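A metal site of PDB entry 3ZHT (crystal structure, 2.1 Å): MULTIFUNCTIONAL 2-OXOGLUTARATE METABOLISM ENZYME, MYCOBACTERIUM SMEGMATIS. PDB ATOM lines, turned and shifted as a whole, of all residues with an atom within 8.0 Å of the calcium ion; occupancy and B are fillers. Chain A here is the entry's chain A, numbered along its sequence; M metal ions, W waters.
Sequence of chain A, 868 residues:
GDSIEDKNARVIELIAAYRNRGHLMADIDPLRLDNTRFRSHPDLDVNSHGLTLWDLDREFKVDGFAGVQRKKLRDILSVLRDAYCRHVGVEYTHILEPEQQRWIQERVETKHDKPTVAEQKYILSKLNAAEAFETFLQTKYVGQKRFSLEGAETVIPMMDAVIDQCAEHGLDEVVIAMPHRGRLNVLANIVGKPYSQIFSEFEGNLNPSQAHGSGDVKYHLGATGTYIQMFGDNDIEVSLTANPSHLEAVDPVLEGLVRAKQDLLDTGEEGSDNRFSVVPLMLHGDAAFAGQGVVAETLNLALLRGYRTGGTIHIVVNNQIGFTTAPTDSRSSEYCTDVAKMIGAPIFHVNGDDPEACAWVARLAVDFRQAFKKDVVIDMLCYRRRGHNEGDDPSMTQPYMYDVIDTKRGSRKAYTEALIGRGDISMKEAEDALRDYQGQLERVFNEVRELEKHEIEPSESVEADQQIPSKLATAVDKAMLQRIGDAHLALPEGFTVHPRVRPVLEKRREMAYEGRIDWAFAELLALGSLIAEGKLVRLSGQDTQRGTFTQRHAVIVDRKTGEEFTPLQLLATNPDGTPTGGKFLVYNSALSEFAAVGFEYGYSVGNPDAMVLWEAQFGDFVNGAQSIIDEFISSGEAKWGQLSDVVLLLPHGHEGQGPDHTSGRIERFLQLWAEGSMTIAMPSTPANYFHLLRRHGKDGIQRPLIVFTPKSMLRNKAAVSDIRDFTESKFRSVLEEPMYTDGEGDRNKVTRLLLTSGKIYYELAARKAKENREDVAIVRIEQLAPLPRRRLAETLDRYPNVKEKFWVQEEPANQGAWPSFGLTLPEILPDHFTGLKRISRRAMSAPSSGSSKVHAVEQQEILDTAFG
OD1 of Asp 645 lies close to N of Arg 703 (3.0 Å).
Water W1 bridges OD2 of Asp 699 (2.6 Å) and ND1 of His 696 (3.0 Å).
Four residues have an atom within 4 Å of the calcium ion: Asp 645, His 696, Asp 699 and Ile 701. The nearest printed residue that does not touch the calcium ion is Gln 702 (4.5 Å).
The backbone carbonyl oxygen (O) of Ile 701 binds the calcium ion (2.3 Å). The backbone carbonyl oxygen (O) of His 696 is bound to the calcium ion (2.4 Å). The side-chain carboxylate (OD2) of Asp 645 is bound to the calcium ion, 2.4 Å away. The calcium ion is bound by OD1 of Asp 699, at 2.5 Å. The calcium ion is bound by water W1 (2.5 Å). The side-chain carboxylate (OD1) of Asp 645 is bound to the calcium ion, 2.5 Å away. Water W2 binds the calcium ion, at 2.6 Å.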
ATOM      1  N   LYS A 535     -26.637   0.627  -4.459  1.00  0.00           N
ATOM      2  CA  LYS A 535     -25.993   1.040  -5.703  1.00  0.00           C
ATOM      3  C   LYS A 535     -24.702   1.811  -5.479  1.00  0.00           C
ATOM      4  O   LYS A 535     -24.616   2.645  -4.589  1.00  0.00           O
ATOM      5  CB  LYS A 535     -26.954   1.908  -6.538  1.00  0.00           C
ATOM      6  CG  LYS A 535     -26.614   1.944  -8.025  1.00  0.00           C
ATOM      7  CD  LYS A 535     -27.792   2.343  -8.860  1.00  0.00           C
ATOM      8  CE  LYS A 535     -27.504   2.118 -10.313  1.00  0.00           C
ATOM      9  NZ  LYS A 535     -27.637   0.686 -10.677  1.00  0.00           N
ATOM     10  N   PRO A 608     -21.696  -1.902 -15.426  1.00  0.00           N
ATOM     11  CA  PRO A 608     -23.063  -1.519 -15.849  1.00  0.00           C
ATOM     12  C   PRO A 608     -24.026  -1.276 -14.682  1.00  0.00           C
ATOM     13  O   PRO A 608     -25.079  -0.697 -14.887  1.00  0.00           O
ATOM     14  CB  PRO A 608     -23.532  -2.729 -16.686  1.00  0.00           C
ATOM     15  CG  PRO A 608     -22.320  -3.470 -17.029  1.00  0.00           C
ATOM     16  CD  PRO A 608     -21.340  -3.253 -15.916  1.00  0.00           C
ATOM     17  N   ALA A 610     -23.210   0.395 -11.915  1.00  0.00           N
ATOM     18  CA  ALA A 610     -22.916   1.677 -11.273  1.00  0.00           C
ATOM     19  C   ALA A 610     -23.757   2.803 -11.826  1.00  0.00           C
ATOM     20  O   ALA A 610     -24.133   2.780 -12.996  1.00  0.00           O
ATOM     21  CB  ALA A 610     -21.458   2.028 -11.439  1.00  0.00           C
ATOM     22  N   MET A 611     -24.065   3.806 -10.973  1.00  0.00           N
ATOM     23  CA  MET A 611     -24.699   5.068 -11.349  1.00  0.00           C
ATOM     24  C   MET A 611     -23.528   6.006 -11.598  1.00  0.00           C
ATOM     25  O   MET A 611     -22.782   6.280 -10.662  1.00  0.00           O
ATOM     26  CB  MET A 611     -25.662   5.560 -10.234  1.00  0.00           C
ATOM     27  CG  MET A 611     -26.364   6.875 -10.553  1.00  0.00           C
ATOM     28  SD  MET A 611     -27.798   6.701 -11.648  1.00  0.00           S
ATOM     29  CE  MET A 611     -28.384   8.379 -11.620  1.00  0.00           C
ATOM     30  N   SER A 644     -23.672   1.685 -22.431  1.00  0.00           N
ATOM     31  CA  SER A 644     -23.270   2.634 -21.394  1.00  0.00           C
ATOM     32  C   SER A 644     -24.512   3.297 -20.800  1.00  0.00           C
ATOM     33  O   SER A 644     -25.434   3.632 -21.534  1.00  0.00           O
ATOM     34  CB  SER A 644     -22.325   3.673 -21.957  1.00  0.00           C
ATOM     35  OG  SER A 644     -22.016   4.692 -21.015  1.00  0.00           O
ATOM     36  N   ASP A 645     -24.528   3.474 -19.497  1.00  0.00           N
ATOM     37  CA  ASP A 645     -25.599   4.138 -18.769  1.00  0.00           C
ATOM     38  C   ASP A 645     -25.098   5.489 -18.225  1.00  0.00           C
ATOM     39  O   ASP A 645     -25.682   6.011 -17.281  1.00  0.00           O
ATOM     40  CB  ASP A 645     -26.095   3.226 -17.625  1.00  0.00           C
ATOM     41  CG  ASP A 645     -27.576   3.370 -17.322  1.00  0.00           C
ATOM     42  OD1 ASP A 645     -28.345   3.581 -18.275  1.00  0.00           O
ATOM     43  OD2 ASP A 645     -27.957   3.237 -16.139  1.00  0.00           O
ATOM     44  N   VAL A 646     -24.023   6.048 -18.818  1.00  0.00           N
ATOM     45  CA  VAL A 646     -23.410   7.300 -18.349  1.00  0.00           C
ATOM     46  C   VAL A 646     -24.413   8.479 -18.369  1.00  0.00           C
ATOM     47  O   VAL A 646     -25.255   8.570 -19.252  1.00  0.00           O
ATOM     48  CB  VAL A 646     -22.085   7.651 -19.105  1.00  0.00           C
ATOM     49  CG1 VAL A 646     -22.315   8.063 -20.567  1.00  0.00           C
ATOM     50  CG2 VAL A 646     -21.268   8.709 -18.354  1.00  0.00           C
ATOM     51  N   VAL A 647     -24.322   9.357 -17.359  1.00  0.00           N
ATOM     52  CA  VAL A 647     -25.141  10.554 -17.266  1.00  0.00           C
ATOM     53  C   VAL A 647     -24.255  11.764 -17.491  1.00  0.00           C
ATOM     54  O   VAL A 647     -23.222  11.884 -16.828  1.00  0.00           O
ATOM     55  CB  VAL A 647     -25.898  10.685 -15.906  1.00  0.00           C
ATOM     56  CG1 VAL A 647     -26.813  11.914 -15.885  1.00  0.00           C
ATOM     57  CG2 VAL A 647     -26.688   9.422 -15.584  1.00  0.00           C
ATOM     58  N   THR A 679     -31.387   9.107 -23.681  1.00  0.00           N
ATOM     59  CA  THR A 679     -32.513   9.806 -23.065  1.00  0.00           C
ATOM     60  C   THR A 679     -32.032  11.261 -22.913  1.00  0.00           C
ATOM     61  O   THR A 679     -30.894  11.468 -22.485  1.00  0.00           O
ATOM     62  CB  THR A 679     -32.949   9.176 -21.744  1.00  0.00           C
ATOM     63  OG1 THR A 679     -33.202   7.798 -21.945  1.00  0.00           O
ATOM     64  CG2 THR A 679     -34.203   9.864 -21.146  1.00  0.00           C
ATOM     65  N   LEU A 692     -36.223  11.260 -12.389  1.00  0.00           N
ATOM     66  CA  LEU A 692     -35.447  11.032 -13.607  1.00  0.00           C
ATOM     67  C   LEU A 692     -34.159  10.228 -13.299  1.00  0.00           C
ATOM     68  O   LEU A 692     -33.893   9.235 -13.974  1.00  0.00           O
ATOM     69  CB  LEU A 692     -35.095  12.369 -14.297  1.00  0.00           C
ATOM     70  CG  LEU A 692     -34.255  12.281 -15.587  1.00  0.00           C
ATOM     71  CD1 LEU A 692     -35.106  11.880 -16.789  1.00  0.00           C
ATOM     72  CD2 LEU A 692     -33.534  13.573 -15.863  1.00  0.00           C
ATOM     73  N   LEU A 693     -33.408  10.637 -12.265  1.00  0.00           N
ATOM     74  CA  LEU A 693     -32.158   9.966 -11.870  1.00  0.00           C
ATOM     75  C   LEU A 693     -32.426   8.560 -11.320  1.00  0.00           C
ATOM     76  O   LEU A 693     -31.689   7.626 -11.670  1.00  0.00           O
ATOM     77  CB  LEU A 693     -31.368  10.780 -10.820  1.00  0.00           C
ATOM     78  CG  LEU A 693     -30.777  12.125 -11.240  1.00  0.00           C
ATOM     79  CD1 LEU A 693     -30.076  12.785 -10.066  1.00  0.00           C
ATOM     80  CD2 LEU A 693     -29.800  11.968 -12.411  1.00  0.00           C
ATOM     81  N   ARG A 694     -33.470   8.415 -10.486  1.00  0.00           N
ATOM     82  CA  ARG A 694     -33.834   7.117  -9.911  1.00  0.00           C
ATOM     83  C   ARG A 694     -34.341   6.152 -11.004  1.00  0.00           C
ATOM     84  O   ARG A 694     -33.928   4.996 -10.992  1.00  0.00           O
ATOM     85  CB  ARG A 694     -34.850   7.260  -8.767  1.00  0.00           C
ATOM     86  CG  ARG A 694     -34.145   7.671  -7.477  1.00  0.00           C
ATOM     87  CD  ARG A 694     -35.035   7.674  -6.243  1.00  0.00           C
ATOM     88  NE  ARG A 694     -35.756   6.425  -5.983  1.00  0.00           N
ATOM     89  CZ  ARG A 694     -35.206   5.323  -5.490  1.00  0.00           C
ATOM     90  NH1 ARG A 694     -33.907   5.276  -5.207  1.00  0.00           N
ATOM     91  NH2 ARG A 694     -35.941   4.237  -5.291  1.00  0.00           N
ATOM     92  N   ARG A 695     -35.154   6.633 -11.987  1.00  0.00           N
ATOM     93  CA  ARG A 695     -35.610   5.791 -13.097  1.00  0.00           C
ATOM     94  C   ARG A 695     -34.391   5.277 -13.869  1.00  0.00           C
ATOM     95  O   ARG A 695     -34.268   4.084 -14.098  1.00  0.00           O
ATOM     96  CB  ARG A 695     -36.594   6.540 -14.033  1.00  0.00           C
ATOM     97  CG  ARG A 695     -37.106   5.693 -15.217  1.00  0.00           C
ATOM     98  CD  ARG A 695     -37.982   6.467 -16.188  1.00  0.00           C
ATOM     99  NE  ARG A 695     -37.226   7.491 -16.928  1.00  0.00           N
ATOM    100  CZ  ARG A 695     -37.705   8.200 -17.943  1.00  0.00           C
ATOM    101  NH1 ARG A 695     -38.948   8.029 -18.361  1.00  0.00           N
ATOM    102  NH2 ARG A 695     -36.934   9.089 -18.566  1.00  0.00           N
ATOM    103  N   HIS A 696     -33.447   6.198 -14.183  1.00  0.00           N
ATOM    104  CA  HIS A 696     -32.218   5.900 -14.897  1.00  0.00           C
ATOM    105  C   HIS A 696     -31.368   4.837 -14.186  1.00  0.00           C
ATOM    106  O   HIS A 696     -30.868   3.935 -14.843  1.00  0.00           O
ATOM    107  CB  HIS A 696     -31.387   7.177 -15.107  1.00  0.00           C
ATOM    108  CG  HIS A 696     -30.166   6.934 -15.921  1.00  0.00           C
ATOM    109  ND1 HIS A 696     -30.229   6.755 -17.281  1.00  0.00           N
ATOM    110  CD2 HIS A 696     -28.880   6.786 -15.515  1.00  0.00           C
ATOM    111  CE1 HIS A 696     -28.981   6.532 -17.671  1.00  0.00           C
ATOM    112  NE2 HIS A 696     -28.137   6.542 -16.644  1.00  0.00           N
ATOM    113  N   GLY A 697     -31.230   4.949 -12.871  1.00  0.00           N
ATOM    114  CA  GLY A 697     -30.467   3.981 -12.087  1.00  0.00           C
ATOM    115  C   GLY A 697     -31.161   2.652 -11.841  1.00  0.00           C
ATOM    116  O   GLY A 697     -30.489   1.674 -11.530  1.00  0.00           O
ATOM    117  N   LYS A 698     -32.500   2.586 -11.963  1.00  0.00           N
ATOM    118  CA  LYS A 698     -33.244   1.343 -11.628  1.00  0.00           C
ATOM    119  C   LYS A 698     -33.970   0.664 -12.809  1.00  0.00           C
ATOM    120  O   LYS A 698     -34.532  -0.412 -12.606  1.00  0.00           O
ATOM    121  CB  LYS A 698     -34.302   1.661 -10.548  1.00  0.00           C
ATOM    122  CG  LYS A 698     -33.750   2.183  -9.227  1.00  0.00           C
ATOM    123  CD  LYS A 698     -34.830   2.742  -8.298  1.00  0.00           C
ATOM    124  CE  LYS A 698     -35.695   1.660  -7.648  1.00  0.00           C
ATOM    125  NZ  LYS A 698     -34.896   0.784  -6.755  1.00  0.00           N
ATOM    126  N   ASP A 699     -33.997   1.274 -14.013  1.00  0.00           N
ATOM    127  CA  ASP A 699     -34.744   0.731 -15.167  1.00  0.00           C
ATOM    128  C   ASP A 699     -34.139  -0.547 -15.794  1.00  0.00           C
ATOM    129  O   ASP A 699     -34.783  -1.143 -16.664  1.00  0.00           O
ATOM    130  CB  ASP A 699     -34.915   1.809 -16.263  1.00  0.00           C
ATOM    131  CG  ASP A 699     -33.620   2.399 -16.803  1.00  0.00           C
ATOM    132  OD1 ASP A 699     -32.541   1.868 -16.486  1.00  0.00           O
ATOM    133  OD2 ASP A 699     -33.698   3.401 -17.553  1.00  0.00           O
ATOM    134  N   GLY A 700     -32.933  -0.922 -15.397  1.00  0.00           N
ATOM    135  CA  GLY A 700     -32.256  -2.112 -15.927  1.00  0.00           C
ATOM    136  C   GLY A 700     -31.863  -2.000 -17.387  1.00  0.00           C
ATOM    137  O   GLY A 700     -31.615  -3.023 -18.036  1.00  0.00           O
ATOM    138  N   ILE A 701     -31.829  -0.753 -17.935  1.00  0.00           N
ATOM    139  CA  ILE A 701     -31.514  -0.430 -19.322  1.00  0.00           C
ATOM    140  C   ILE A 701     -30.225   0.375 -19.330  1.00  0.00           C
ATOM    141  O   ILE A 701     -30.107   1.317 -18.551  1.00  0.00           O
ATOM    142  CB  ILE A 701     -32.713   0.325 -19.990  1.00  0.00           C
ATOM    143  CG1 ILE A 701     -33.893  -0.637 -20.267  1.00  0.00           C
ATOM    144  CG2 ILE A 701     -32.312   1.075 -21.277  1.00  0.00           C
ATOM    145  CD1 ILE A 701     -35.274  -0.011 -19.994  1.00  0.00           C
ATOM    146  N   GLN A 702     -29.291   0.007 -20.202  1.00  0.00           N
ATOM    147  CA  GLN A 702     -28.011   0.684 -20.313  1.00  0.00           C
ATOM    148  C   GLN A 702     -28.062   1.644 -21.494  1.00  0.00           C
ATOM    149  O   GLN A 702     -27.787   1.287 -22.656  1.00  0.00           O
ATOM    150  CB  GLN A 702     -26.845  -0.311 -20.392  1.00  0.00           C
ATOM    151  CG  GLN A 702     -26.806  -1.341 -19.254  1.00  0.00           C
ATOM    152  CD  GLN A 702     -26.522  -0.701 -17.925  1.00  0.00           C
ATOM    153  OE1 GLN A 702     -25.459  -0.104 -17.737  1.00  0.00           O
ATOM    154  NE2 GLN A 702     -27.442  -0.817 -16.977  1.00  0.00           N
ATOM    155  N   ARG A 703     -28.442   2.895 -21.167  1.00  0.00           N
ATOM    156  CA  ARG A 703     -28.623   3.981 -22.124  1.00  0.00           C
ATOM    157  C   ARG A 703     -28.086   5.305 -21.551  1.00  0.00           C
ATOM    158  O   ARG A 703     -28.487   5.668 -20.440  1.00  0.00           O
ATOM    159  CB  ARG A 703     -30.132   4.094 -22.397  1.00  0.00           C
ATOM    160  CG  ARG A 703     -30.566   4.758 -23.688  1.00  0.00           C
ATOM    161  CD  ARG A 703     -30.464   3.834 -24.896  1.00  0.00           C
ATOM    162  NE  ARG A 703     -31.030   2.483 -24.759  1.00  0.00           N
ATOM    163  CZ  ARG A 703     -32.327   2.194 -24.859  1.00  0.00           C
ATOM    164  NH1 ARG A 703     -33.228   3.149 -25.035  1.00  0.00           N
ATOM    165  NH2 ARG A 703     -32.735   0.931 -24.748  1.00  0.00           N
ATOM    166  N   PRO A 704     -27.257   6.089 -22.274  1.00  0.00           N
ATOM    167  CA  PRO A 704     -26.830   7.387 -21.715  1.00  0.00           C
ATOM    168  C   PRO A 704     -28.002   8.359 -21.487  1.00  0.00           C
ATOM    169  O   PRO A 704     -29.015   8.334 -22.182  1.00  0.00           O
ATOM    170  CB  PRO A 704     -25.853   7.930 -22.767  1.00  0.00           C
ATOM    171  CG  PRO A 704     -25.454   6.718 -23.593  1.00  0.00           C
ATOM    172  CD  PRO A 704     -26.665   5.843 -23.604  1.00  0.00           C
ATOM    173  N   LEU A 705     -27.865   9.167 -20.456  1.00  0.00           N
ATOM    174  CA  LEU A 705     -28.846  10.168 -20.108  1.00  0.00           C
ATOM    175  C   LEU A 705     -28.176  11.535 -20.189  1.00  0.00           C
ATOM    176  O   LEU A 705     -27.128  11.735 -19.573  1.00  0.00           O
ATOM    177  CB  LEU A 705     -29.449   9.888 -18.707  1.00  0.00           C
ATOM    178  CG  LEU A 705     -30.273  11.003 -18.021  1.00  0.00           C
ATOM    179  CD1 LEU A 705     -31.591  11.264 -18.731  1.00  0.00           C
ATOM    180  CD2 LEU A 705     -30.526  10.672 -16.563  1.00  0.00           C
HETATM  181 CA    CA M   1     -30.250   2.781 -16.812  1.00  0.00          CA
HETATM  182  O   HOH W   1     -31.379   4.232 -18.517  1.00  0.00           O
HETATM  183  O   HOH W   2     -29.569   0.945 -15.127  1.00  0.00           O
